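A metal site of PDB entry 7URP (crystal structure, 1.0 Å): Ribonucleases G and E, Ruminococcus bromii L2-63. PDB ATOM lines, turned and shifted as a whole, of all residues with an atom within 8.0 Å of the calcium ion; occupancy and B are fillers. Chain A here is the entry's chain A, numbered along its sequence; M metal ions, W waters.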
ATOM      1  N   ALA A   1      18.287  17.615 -31.297  1.00  0.00           N
ATOM      2  CA  ALA A   1      17.855  16.819 -30.106  1.00  0.00           C
ATOM      3  C   ALA A   1      17.339  17.755 -29.012  1.00  0.00           C
ATOM      4  O   ALA A   1      17.901  18.851 -28.811  1.00  0.00           O
ATOM      5  CB  ALA A   1      19.005  15.966 -29.604  1.00  0.00           C
ATOM      6  N   VAL A   2      16.294  17.321 -28.285  1.00  0.00           N
ATOM      7  CA  VAL A   2      15.723  18.146 -27.187  1.00  0.00           C
ATOM      8  C   VAL A   2      16.506  17.883 -25.877  1.00  0.00           C
ATOM      9  O   VAL A   2      16.431  18.764 -24.988  1.00  0.00           O
ATOM     10  CB  VAL A   2      14.203  17.945 -27.081  1.00  0.00           C
ATOM     11  CG1 VAL A   2      13.577  18.546 -25.836  1.00  0.00           C
ATOM     12  CG2 VAL A   2      13.506  18.487 -28.310  1.00  0.00           C
ATOM     13  N   ASP A   3      17.213  16.751 -25.761  1.00  0.00           N
ATOM     14  CA  ASP A   3      18.172  16.453 -24.653  1.00  0.00           C
ATOM     15  C   ASP A   3      19.328  17.450 -24.666  1.00  0.00           C
ATOM     16  O   ASP A   3      19.594  18.025 -25.711  1.00  0.00           O
ATOM     17  CB  ASP A   3      18.753  15.030 -24.750  1.00  0.00           C
ATOM     18  CG  ASP A   3      17.783  13.892 -24.494  1.00  0.00           C
ATOM     19  OD1 ASP A   3      16.576  14.163 -24.379  1.00  0.00           O
ATOM     20  OD2 ASP A   3      18.249  12.742 -24.447  1.00  0.00           O
ATOM     21  N   ASN A   4      19.974  17.617 -23.523  1.00  0.00           N
ATOM     22  CA  ASN A   4      20.913  18.735 -23.311  1.00  0.00           C
ATOM     23  C   ASN A   4      22.328  18.227 -23.109  1.00  0.00           C
ATOM     24  O   ASN A   4      22.560  17.032 -22.895  1.00  0.00           O
ATOM     25  CB  ASN A   4      20.456  19.554 -22.125  1.00  0.00           C
ATOM     26  CG  ASN A   4      19.084  20.148 -22.377  1.00  0.00           C
ATOM     27  OD1 ASN A   4      18.767  20.496 -23.516  1.00  0.00           O
ATOM     28  ND2 ASN A   4      18.333  20.334 -21.321  1.00  0.00           N
ATOM     29  N   LEU A   5      23.256  19.172 -23.144  1.00  0.00           N
ATOM     30  CA  LEU A   5      24.675  18.909 -22.831  1.00  0.00           C
ATOM     31  C   LEU A   5      25.053  19.712 -21.579  1.00  0.00           C
ATOM     32  O   LEU A   5      24.869  20.942 -21.548  1.00  0.00           O
ATOM     33  CB  LEU A   5      25.589  19.329 -23.987  1.00  0.00           C
ATOM     34  CG  LEU A   5      27.056  18.993 -23.790  1.00  0.00           C
ATOM     35  CD1 LEU A   5      27.304  17.484 -23.746  1.00  0.00           C
ATOM     36  CD2 LEU A   5      27.896  19.606 -24.884  1.00  0.00           C
ATOM     37  N   THR A  21      24.441  23.880 -18.341  1.00  0.00           N
ATOM     38  CA  THR A  21      23.674  22.937 -19.178  1.00  0.00           C
ATOM     39  C   THR A  21      22.983  23.711 -20.282  1.00  0.00           C
ATOM     40  O   THR A  21      22.373  24.749 -20.005  1.00  0.00           O
ATOM     41  CB  THR A  21      22.722  22.120 -18.320  1.00  0.00           C
ATOM     42  OG1 THR A  21      23.504  21.383 -17.377  1.00  0.00           O
ATOM     43  CG2 THR A  21      21.884  21.182 -19.147  1.00  0.00           C
ATOM     44  N   PHE A  22      23.044  23.171 -21.500  1.00  0.00           N
ATOM     45  CA  PHE A  22      22.660  23.918 -22.720  1.00  0.00           C
ATOM     46  C   PHE A  22      21.918  23.027 -23.698  1.00  0.00           C
ATOM     47  O   PHE A  22      22.089  21.817 -23.712  1.00  0.00           O
ATOM     48  CB  PHE A  22      23.901  24.488 -23.392  1.00  0.00           C
ATOM     49  CG  PHE A  22      24.698  25.363 -22.472  1.00  0.00           C
ATOM     50  CD1 PHE A  22      24.331  26.691 -22.316  1.00  0.00           C
ATOM     51  CD2 PHE A  22      25.756  24.857 -21.727  1.00  0.00           C
ATOM     52  CE1 PHE A  22      25.032  27.507 -21.448  1.00  0.00           C
ATOM     53  CE2 PHE A  22      26.462  25.683 -20.851  1.00  0.00           C
ATOM     54  CZ  PHE A  22      26.085  26.991 -20.712  1.00  0.00           C
ATOM     55  N   ASN A  23      21.124  23.692 -24.518  1.00  0.00           N
ATOM     56  CA  ASN A  23      20.432  23.030 -25.636  1.00  0.00           C
ATOM     57  C   ASN A  23      21.424  22.730 -26.757  1.00  0.00           C
ATOM     58  O   ASN A  23      22.352  23.509 -27.007  1.00  0.00           O
ATOM     59  CB  ASN A  23      19.309  23.901 -26.190  1.00  0.00           C
ATOM     60  CG  ASN A  23      18.226  24.161 -25.172  1.00  0.00           C
ATOM     61  OD1 ASN A  23      17.632  23.217 -24.648  1.00  0.00           O
ATOM     62  ND2 ASN A  23      17.935  25.427 -24.907  1.00  0.00           N
ATOM     63  N   VAL A  24      21.163  21.651 -27.480  1.00  0.00           N
ATOM     64  CA  VAL A  24      21.828  21.386 -28.775  1.00  0.00           C
ATOM     65  C   VAL A  24      21.608  22.612 -29.667  1.00  0.00           C
ATOM     66  O   VAL A  24      20.471  23.121 -29.738  1.00  0.00           O
ATOM     67  CB  VAL A  24      21.324  20.082 -29.401  1.00  0.00           C
ATOM     68  CG1 VAL A  24      21.905  19.888 -30.786  1.00  0.00           C
ATOM     69  CG2 VAL A  24      21.660  18.900 -28.510  1.00  0.00           C
ATOM     70  N   ASP A  26      23.091  25.538 -29.120  1.00  0.00           N
ATOM     71  CA  ASP A  26      23.465  26.742 -28.342  1.00  0.00           C
ATOM     72  C   ASP A  26      24.948  27.039 -28.548  1.00  0.00           C
ATOM     73  O   ASP A  26      25.766  26.119 -28.694  1.00  0.00           O
ATOM     74  CB  ASP A  26      23.195  26.575 -26.843  1.00  0.00           C
ATOM     75  CG  ASP A  26      21.745  26.720 -26.392  1.00  0.00           C
ATOM     76  OD1 ASP A  26      20.900  27.095 -27.239  1.00  0.00           O
ATOM     77  OD2 ASP A  26      21.476  26.461 -25.190  1.00  0.00           O
ATOM     78  N   THR A 103      24.948  15.537 -26.744  1.00  0.00           N
ATOM     79  CA  THR A 103      24.231  15.560 -25.463  1.00  0.00           C
ATOM     80  C   THR A 103      24.986  14.725 -24.428  1.00  0.00           C
ATOM     81  O   THR A 103      25.908  13.960 -24.808  1.00  0.00           O
ATOM     82  CB  THR A 103      22.799  15.056 -25.654  1.00  0.00           C
ATOM     83  OG1 THR A 103      22.855  13.684 -26.050  1.00  0.00           O
ATOM     84  CG2 THR A 103      22.031  15.864 -26.683  1.00  0.00           C
HETATM   85 CA    CA M   1      16.932  21.028 -24.882  1.00  0.00          CA
HETATM   86  O   HOH W   1      15.907  21.673 -26.931  1.00  0.00           O
HETATM   87  O   HOH W   2      18.599  20.318 -26.560  1.00  0.00           O
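The side-chain carboxylate (OD2) of Asp 26 is in hydrogen-bond range of the backbone NH (N) of Asn 23 (2.9 Å).
Within 4 Å of the calcium ion: Val 2, Asn 4 and Asn 23.
Water W2 lies within hydrogen-bond range of O of Asp 3 (2.6 Å), O of Ala 1 (2.8 Å) and N of Val 24 (3.0 Å).
The calcium ion is bound by OD1 of Asn 23. The backbone carbonyl oxygen (O) of Val 2 binds the calcium ion (2.3 Å). The calcium ion is bound by OD1 of Asn 4, 2.3 Å away. The calcium ion is bound by water W1 (2.4 Å). The calcium ion is bound by water W2, 2.5 Å away.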
